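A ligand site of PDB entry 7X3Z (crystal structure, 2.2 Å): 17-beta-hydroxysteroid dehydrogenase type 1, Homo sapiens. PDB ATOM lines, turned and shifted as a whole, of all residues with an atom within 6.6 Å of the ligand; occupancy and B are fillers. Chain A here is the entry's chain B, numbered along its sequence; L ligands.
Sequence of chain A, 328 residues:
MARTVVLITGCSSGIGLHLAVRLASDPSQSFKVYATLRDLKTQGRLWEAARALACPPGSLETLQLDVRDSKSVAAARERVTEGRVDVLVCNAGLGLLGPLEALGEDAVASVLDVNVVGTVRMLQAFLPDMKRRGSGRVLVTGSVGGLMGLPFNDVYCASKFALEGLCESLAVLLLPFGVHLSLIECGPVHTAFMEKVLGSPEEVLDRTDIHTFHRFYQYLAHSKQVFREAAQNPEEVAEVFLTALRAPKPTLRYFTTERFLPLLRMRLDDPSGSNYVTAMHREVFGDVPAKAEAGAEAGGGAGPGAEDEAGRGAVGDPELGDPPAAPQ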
ATOM      1  N   SER A 143     -14.109  -1.004  18.409  1.00  0.00           N
ATOM      2  CA  SER A 143     -15.563  -0.971  18.463  1.00  0.00           C
ATOM      3  C   SER A 143     -16.092  -0.346  17.177  1.00  0.00           C
ATOM      4  O   SER A 143     -15.460   0.535  16.589  1.00  0.00           O
ATOM      5  CB  SER A 143     -16.081  -0.240  19.660  1.00  0.00           C
ATOM      6  OG  SER A 143     -17.509  -0.097  19.627  1.00  0.00           O
ATOM      7  N   VAL A 144     -17.266  -0.845  16.771  1.00  0.00           N
ATOM      8  CA  VAL A 144     -18.064  -0.180  15.763  1.00  0.00           C
ATOM      9  C   VAL A 144     -18.299   1.289  16.157  1.00  0.00           C
ATOM     10  O   VAL A 144     -18.281   2.125  15.276  1.00  0.00           O
ATOM     11  CB  VAL A 144     -19.382  -0.954  15.494  1.00  0.00           C
ATOM     12  CG1 VAL A 144     -20.221  -1.138  16.740  1.00  0.00           C
ATOM     13  CG2 VAL A 144     -20.245  -0.269  14.441  1.00  0.00           C
ATOM     14  N   GLY A 145     -18.508   1.610  17.441  1.00  0.00           N
ATOM     15  CA  GLY A 145     -18.548   2.976  17.963  1.00  0.00           C
ATOM     16  C   GLY A 145     -17.247   3.785  17.727  1.00  0.00           C
ATOM     17  O   GLY A 145     -17.174   4.956  18.083  1.00  0.00           O
ATOM     18  N   MET A 148     -18.180   4.682  13.655  1.00  0.00           N
ATOM     19  CA  MET A 148     -19.333   5.487  13.377  1.00  0.00           C
ATOM     20  C   MET A 148     -19.881   6.015  14.693  1.00  0.00           C
ATOM     21  O   MET A 148     -19.916   5.287  15.682  1.00  0.00           O
ATOM     22  CB  MET A 148     -20.383   4.631  12.661  1.00  0.00           C
ATOM     23  CG  MET A 148     -20.991   3.534  13.544  1.00  0.00           C
ATOM     24  SD  MET A 148     -22.034   2.393  12.597  1.00  0.00           S
ATOM     25  CE  MET A 148     -20.753   1.568  11.650  1.00  0.00           C
ATOM     26  N   LEU A 150     -22.333   7.197  17.648  1.00  0.00           N
ATOM     27  CA  LEU A 150     -23.531   6.652  18.258  1.00  0.00           C
ATOM     28  C   LEU A 150     -24.084   7.657  19.241  1.00  0.00           C
ATOM     29  O   LEU A 150     -23.386   8.072  20.147  1.00  0.00           O
ATOM     30  CB  LEU A 150     -23.222   5.363  19.019  1.00  0.00           C
ATOM     31  CG  LEU A 150     -22.270   4.381  18.355  1.00  0.00           C
ATOM     32  CD1 LEU A 150     -22.096   3.136  19.241  1.00  0.00           C
ATOM     33  CD2 LEU A 150     -22.736   3.992  16.963  1.00  0.00           C
ATOM     34  N   PRO A 151     -25.394   7.975  19.197  1.00  0.00           N
ATOM     35  CA  PRO A 151     -25.963   9.012  20.065  1.00  0.00           C
ATOM     36  C   PRO A 151     -25.965   8.541  21.512  1.00  0.00           C
ATOM     37  O   PRO A 151     -26.011   7.337  21.788  1.00  0.00           O
ATOM     38  CB  PRO A 151     -27.376   9.244  19.513  1.00  0.00           C
ATOM     39  CG  PRO A 151     -27.729   7.884  18.876  1.00  0.00           C
ATOM     40  CD  PRO A 151     -26.416   7.300  18.370  1.00  0.00           C
ATOM     41  N   ASN A 153     -23.559   8.183  23.255  1.00  0.00           N
ATOM     42  CA  ASN A 153     -22.276   7.550  23.585  1.00  0.00           C
ATOM     43  C   ASN A 153     -21.096   8.433  23.125  1.00  0.00           C
ATOM     44  O   ASN A 153     -20.100   7.950  22.585  1.00  0.00           O
ATOM     45  CB  ASN A 153     -22.180   6.151  22.973  1.00  0.00           C
ATOM     46  CG  ASN A 153     -23.096   5.163  23.665  1.00  0.00           C
ATOM     47  OD1 ASN A 153     -24.290   5.085  23.348  1.00  0.00           O
ATOM     48  ND2 ASN A 153     -22.556   4.445  24.643  1.00  0.00           N
ATOM     49  N   TYR A 156     -17.613   7.789  24.871  1.00  0.00           N
ATOM     50  CA  TYR A 156     -17.187   6.440  24.531  1.00  0.00           C
ATOM     51  C   TYR A 156     -16.641   6.399  23.095  1.00  0.00           C
ATOM     52  O   TYR A 156     -15.578   5.840  22.814  1.00  0.00           O
ATOM     53  CB  TYR A 156     -18.353   5.468  24.693  1.00  0.00           C
ATOM     54  CG  TYR A 156     -18.026   4.058  24.300  1.00  0.00           C
ATOM     55  CD1 TYR A 156     -17.202   3.270  25.083  1.00  0.00           C
ATOM     56  CD2 TYR A 156     -18.487   3.542  23.102  1.00  0.00           C
ATOM     57  CE1 TYR A 156     -16.868   1.966  24.707  1.00  0.00           C
ATOM     58  CE2 TYR A 156     -18.162   2.253  22.712  1.00  0.00           C
ATOM     59  CZ  TYR A 156     -17.360   1.464  23.523  1.00  0.00           C
ATOM     60  OH  TYR A 156     -17.024   0.216  23.106  1.00  0.00           O
ATOM     61  N   CYS A 186     -15.418  -4.709  17.881  1.00  0.00           N
ATOM     62  CA  CYS A 186     -16.511  -5.367  18.536  1.00  0.00           C
ATOM     63  C   CYS A 186     -17.782  -4.627  18.178  1.00  0.00           C
ATOM     64  O   CYS A 186     -17.762  -3.416  17.928  1.00  0.00           O
ATOM     65  CB  CYS A 186     -16.204  -5.402  20.022  1.00  0.00           C
ATOM     66  SG  CYS A 186     -14.663  -6.291  20.333  1.00  0.00           S
ATOM     67  N   GLY A 187     -18.885  -5.360  18.093  1.00  0.00           N
ATOM     68  CA  GLY A 187     -20.183  -4.747  18.250  1.00  0.00           C
ATOM     69  C   GLY A 187     -20.488  -4.722  19.731  1.00  0.00           C
ATOM     70  O   GLY A 187     -19.579  -4.869  20.527  1.00  0.00           O
ATOM     71  N   PRO A 188     -21.766  -4.608  20.149  1.00  0.00           N
ATOM     72  CA  PRO A 188     -22.146  -4.846  21.531  1.00  0.00           C
ATOM     73  C   PRO A 188     -21.761  -6.244  21.997  1.00  0.00           C
ATOM     74  O   PRO A 188     -21.593  -7.139  21.176  1.00  0.00           O
ATOM     75  CB  PRO A 188     -23.686  -4.712  21.550  1.00  0.00           C
ATOM     76  CG  PRO A 188     -24.093  -4.832  20.086  1.00  0.00           C
ATOM     77  CD  PRO A 188     -22.926  -4.276  19.297  1.00  0.00           C
ATOM     78  N   VAL A 189     -21.655  -6.406  23.325  1.00  0.00           N
ATOM     79  CA  VAL A 189     -21.108  -7.609  23.924  1.00  0.00           C
ATOM     80  C   VAL A 189     -21.782  -7.814  25.279  1.00  0.00           C
ATOM     81  O   VAL A 189     -21.890  -6.855  26.042  1.00  0.00           O
ATOM     82  CB  VAL A 189     -19.569  -7.528  24.028  1.00  0.00           C
ATOM     83  CG1 VAL A 189     -18.984  -8.563  24.983  1.00  0.00           C
ATOM     84  CG2 VAL A 189     -18.891  -7.631  22.668  1.00  0.00           C
ATOM     85  N   TYR A 219     -33.955   6.082  23.065  1.00  0.00           N
ATOM     86  CA  TYR A 219     -32.657   5.425  22.869  1.00  0.00           C
ATOM     87  C   TYR A 219     -32.485   4.193  23.762  1.00  0.00           C
ATOM     88  O   TYR A 219     -32.014   3.140  23.301  1.00  0.00           O
ATOM     89  CB  TYR A 219     -31.508   6.417  23.126  1.00  0.00           C
ATOM     90  CG  TYR A 219     -30.186   5.700  23.139  1.00  0.00           C
ATOM     91  CD1 TYR A 219     -29.541   5.428  21.952  1.00  0.00           C
ATOM     92  CD2 TYR A 219     -29.736   5.093  24.308  1.00  0.00           C
ATOM     93  CE1 TYR A 219     -28.401   4.654  21.930  1.00  0.00           C
ATOM     94  CE2 TYR A 219     -28.592   4.325  24.304  1.00  0.00           C
ATOM     95  CZ  TYR A 219     -27.914   4.119  23.109  1.00  0.00           C
ATOM     96  OH  TYR A 219     -26.796   3.349  23.091  1.00  0.00           O
ATOM     97  N   HIS A 222     -34.660   1.474  22.697  1.00  0.00           N
ATOM     98  CA  HIS A 222     -34.198   0.975  21.414  1.00  0.00           C
ATOM     99  C   HIS A 222     -32.989   0.076  21.580  1.00  0.00           C
ATOM    100  O   HIS A 222     -32.931  -0.988  20.962  1.00  0.00           O
ATOM    101  CB  HIS A 222     -33.850   2.061  20.402  1.00  0.00           C
ATOM    102  CG  HIS A 222     -33.346   1.454  19.145  1.00  0.00           C
ATOM    103  ND1 HIS A 222     -34.171   0.804  18.241  1.00  0.00           N
ATOM    104  CD2 HIS A 222     -32.102   1.331  18.653  1.00  0.00           C
ATOM    105  CE1 HIS A 222     -33.447   0.313  17.250  1.00  0.00           C
ATOM    106  NE2 HIS A 222     -32.196   0.611  17.479  1.00  0.00           N
ATOM    107  N   SER A 223     -32.008   0.498  22.383  1.00  0.00           N
ATOM    108  CA  SER A 223     -30.719  -0.188  22.394  1.00  0.00           C
ATOM    109  C   SER A 223     -30.771  -1.452  23.243  1.00  0.00           C
ATOM    110  O   SER A 223     -30.037  -2.379  22.926  1.00  0.00           O
ATOM    111  CB  SER A 223     -29.592   0.722  22.803  1.00  0.00           C
ATOM    112  OG  SER A 223     -29.554   0.840  24.215  1.00  0.00           O
ATOM    113  N   LYS A 224     -31.638  -1.522  24.284  1.00  0.00           N
ATOM    114  CA  LYS A 224     -31.929  -2.783  24.984  1.00  0.00           C
ATOM    115  C   LYS A 224     -32.131  -3.896  23.947  1.00  0.00           C
ATOM    116  O   LYS A 224     -31.529  -4.969  24.046  1.00  0.00           O
ATOM    117  CB  LYS A 224     -33.249  -2.837  25.771  1.00  0.00           C
ATOM    118  CG  LYS A 224     -33.431  -1.930  26.980  1.00  0.00           C
ATOM    119  CD  LYS A 224     -32.249  -1.836  27.922  1.00  0.00           C
ATOM    120  CE  LYS A 224     -31.346  -0.658  27.623  1.00  0.00           C
ATOM    121  NZ  LYS A 224     -30.112  -0.696  28.435  1.00  0.00           N
ATOM    122  N   VAL A 226     -31.422  -3.999  20.740  1.00  0.00           N
ATOM    123  CA  VAL A 226     -30.245  -4.373  19.958  1.00  0.00           C
ATOM    124  C   VAL A 226     -29.357  -5.296  20.805  1.00  0.00           C
ATOM    125  O   VAL A 226     -28.794  -6.264  20.272  1.00  0.00           O
ATOM    126  CB  VAL A 226     -29.517  -3.144  19.382  1.00  0.00           C
ATOM    127  CG1 VAL A 226     -28.098  -3.440  18.895  1.00  0.00           C
ATOM    128  CG2 VAL A 226     -30.330  -2.476  18.269  1.00  0.00           C
ATOM    129  N   PHE A 227     -29.260  -5.078  22.125  1.00  0.00           N
ATOM    130  CA  PHE A 227     -28.453  -5.942  22.981  1.00  0.00           C
ATOM    131  C   PHE A 227     -29.058  -7.351  23.080  1.00  0.00           C
ATOM    132  O   PHE A 227     -28.322  -8.331  23.171  1.00  0.00           O
ATOM    133  CB  PHE A 227     -28.214  -5.325  24.361  1.00  0.00           C
ATOM    134  CG  PHE A 227     -26.931  -4.532  24.448  1.00  0.00           C
ATOM    135  CD1 PHE A 227     -25.711  -5.170  24.588  1.00  0.00           C
ATOM    136  CD2 PHE A 227     -26.939  -3.143  24.339  1.00  0.00           C
ATOM    137  CE1 PHE A 227     -24.534  -4.444  24.658  1.00  0.00           C
ATOM    138  CE2 PHE A 227     -25.755  -2.418  24.396  1.00  0.00           C
ATOM    139  CZ  PHE A 227     -24.556  -3.070  24.558  1.00  0.00           C
ATOM    140  N   PHE A 260     -23.488  -4.508  11.146  1.00  0.00           N
ATOM    141  CA  PHE A 260     -23.487  -3.046  11.097  1.00  0.00           C
ATOM    142  C   PHE A 260     -22.682  -2.555   9.896  1.00  0.00           C
ATOM    143  O   PHE A 260     -22.473  -1.359   9.736  1.00  0.00           O
ATOM    144  CB  PHE A 260     -22.982  -2.460  12.424  1.00  0.00           C
ATOM    145  CG  PHE A 260     -23.780  -2.890  13.635  1.00  0.00           C
ATOM    146  CD1 PHE A 260     -25.001  -2.300  13.933  1.00  0.00           C
ATOM    147  CD2 PHE A 260     -23.329  -3.922  14.459  1.00  0.00           C
ATOM    148  CE1 PHE A 260     -25.742  -2.712  15.038  1.00  0.00           C
ATOM    149  CE2 PHE A 260     -24.072  -4.337  15.555  1.00  0.00           C
ATOM    150  CZ  PHE A 260     -25.278  -3.732  15.844  1.00  0.00           C
ATOM    151  N   LEU A 263     -24.922   0.143   7.790  1.00  0.00           N
ATOM    152  CA  LEU A 263     -24.846   1.457   8.411  1.00  0.00           C
ATOM    153  C   LEU A 263     -23.454   2.057   8.256  1.00  0.00           C
ATOM    154  O   LEU A 263     -23.351   3.274   8.124  1.00  0.00           O
ATOM    155  CB  LEU A 263     -25.191   1.322   9.891  1.00  0.00           C
ATOM    156  CG  LEU A 263     -26.663   1.080  10.193  1.00  0.00           C
ATOM    157  CD1 LEU A 263     -26.864   0.713  11.663  1.00  0.00           C
ATOM    158  CD2 LEU A 263     -27.505   2.299   9.810  1.00  0.00           C
ATOM    159  N   MET A 280     -28.638   6.894  10.739  1.00  0.00           N
ATOM    160  CA  MET A 280     -28.474   6.387  12.093  1.00  0.00           C
ATOM    161  C   MET A 280     -29.541   7.011  13.003  1.00  0.00           C
ATOM    162  O   MET A 280     -29.967   6.390  13.973  1.00  0.00           O
ATOM    163  CB  MET A 280     -27.060   6.651  12.641  1.00  0.00           C
ATOM    164  CG  MET A 280     -26.828   6.155  14.072  1.00  0.00           C
ATOM    165  SD  MET A 280     -27.044   4.355  14.384  1.00  0.00           S
ATOM    166  CE  MET A 280     -25.597   3.739  13.533  1.00  0.00           C
ATOM    167  N   GLU A 283     -32.545   4.709  12.168  1.00  0.00           N
ATOM    168  CA  GLU A 283     -32.308   3.370  12.703  1.00  0.00           C
ATOM    169  C   GLU A 283     -32.496   3.338  14.219  1.00  0.00           C
ATOM    170  O   GLU A 283     -33.006   2.372  14.764  1.00  0.00           O
ATOM    171  CB  GLU A 283     -30.909   2.882  12.275  1.00  0.00           C
ATOM    172  CG  GLU A 283     -30.261   1.823  13.169  1.00  0.00           C
ATOM    173  CD  GLU A 283     -30.950   0.475  13.333  1.00  0.00           C
ATOM    174  OE1 GLU A 283     -31.169   0.082  14.502  1.00  0.00           O
ATOM    175  OE2 GLU A 283     -31.215  -0.196  12.313  1.00  0.00           O
ATOM    176  N   VAL A 284     -32.131   4.432  14.878  1.00  0.00           N
ATOM    177  CA  VAL A 284     -32.134   4.480  16.334  1.00  0.00           C
ATOM    178  C   VAL A 284     -33.484   4.950  16.886  1.00  0.00           C
ATOM    179  O   VAL A 284     -33.951   4.434  17.896  1.00  0.00           O
ATOM    180  CB  VAL A 284     -30.973   5.348  16.836  1.00  0.00           C
ATOM    181  CG1 VAL A 284     -31.103   5.628  18.319  1.00  0.00           C
ATOM    182  CG2 VAL A 284     -29.616   4.721  16.485  1.00  0.00           C
HETATM  183  C1  LIG L   1     -24.991  -0.509  19.980  1.00  0.00           C
HETATM  184  C2  LIG L   1     -27.419   0.358  19.855  1.00  0.00           C
HETATM  185  C3  LIG L   1     -27.113   0.966  18.485  1.00  0.00           C
HETATM  186  C4  LIG L   1     -26.775   2.477  18.598  1.00  0.00           C
HETATM  187  O1  LIG L   1     -29.386   1.105  17.616  1.00  0.00           O
HETATM  188  O2  LIG L   1     -20.119  -0.848  22.979  1.00  0.00           O
HETATM  189  C5  LIG L   1     -28.211   0.898  17.428  1.00  0.00           C
HETATM  190  C6  LIG L   1     -27.578   0.561  16.082  1.00  0.00           C
HETATM  191  C7  LIG L   1     -26.066   0.537  16.335  1.00  0.00           C
HETATM  192  C8  LIG L   1     -26.028   0.110  17.811  1.00  0.00           C
HETATM  193  C9  LIG L   1     -24.726   0.087  18.580  1.00  0.00           C
HETATM  194  C10 LIG L   1     -26.152   0.207  20.697  1.00  0.00           C
HETATM  195  C11 LIG L   1     -23.647  -0.732  17.885  1.00  0.00           C
HETATM  196  C12 LIG L   1     -22.324  -0.663  18.639  1.00  0.00           C
HETATM  197  C13 LIG L   1     -22.443  -0.681  20.145  1.00  0.00           C
HETATM  198  C14 LIG L   1     -23.690  -0.601  20.783  1.00  0.00           C
HETATM  199  C15 LIG L   1     -21.255  -0.768  20.876  1.00  0.00           C
HETATM  200  C16 LIG L   1     -21.271  -0.755  22.260  1.00  0.00           C
HETATM  201  C17 LIG L   1     -22.488  -0.666  22.931  1.00  0.00           C
HETATM  202  C18 LIG L   1     -23.675  -0.591  22.193  1.00  0.00           C
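A ring nitrogen (NE2) of His 222 lies within hydrogen-bond range of an oxygen (O1) of the ligand (2.9 Å). The side-chain hydroxyl of Tyr 156 sits at hydrogen-bond distance from an oxygen (O2) of the ligand.
CG1 of Val 144 touches C12 of the ligand, at 2.9 Å. CD1 of Leu 150 touches C12 of the ligand (3.9 Å). CD of Pro 188 touches C12 of the ligand (3.7 Å). Ser 223 touches the ligand. Val 226 touches the ligand. Phe 227 touches the ligand. Phe 260 touches the ligand. Glu 283 touches the ligand (OE1 to O1, 3.7 Å). Val 284 touches the ligand (CG2 to O1, 3.8 Å). Hydrophobic or aromatic side chains that line the ligand: Val 144, Leu 150, Tyr 156, Pro 188, His 222, Val 226, Phe 227, Phe 260 and Val 284. 11 residues have an atom within 4 Å of the ligand: Val 144, Leu 150, Tyr 156, Pro 188, His 222, Ser 223, Val 226, Phe 227, Phe 260, Glu 283 and Val 284.
OE1 of Glu 283 sits at hydrogen-bond distance from NE2 of His 222. O of Cys 186 is in hydrogen-bond range of N of Val 144 (2.9 Å). OG of Ser 223 lies close to O of Tyr 219 (3.5 Å).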
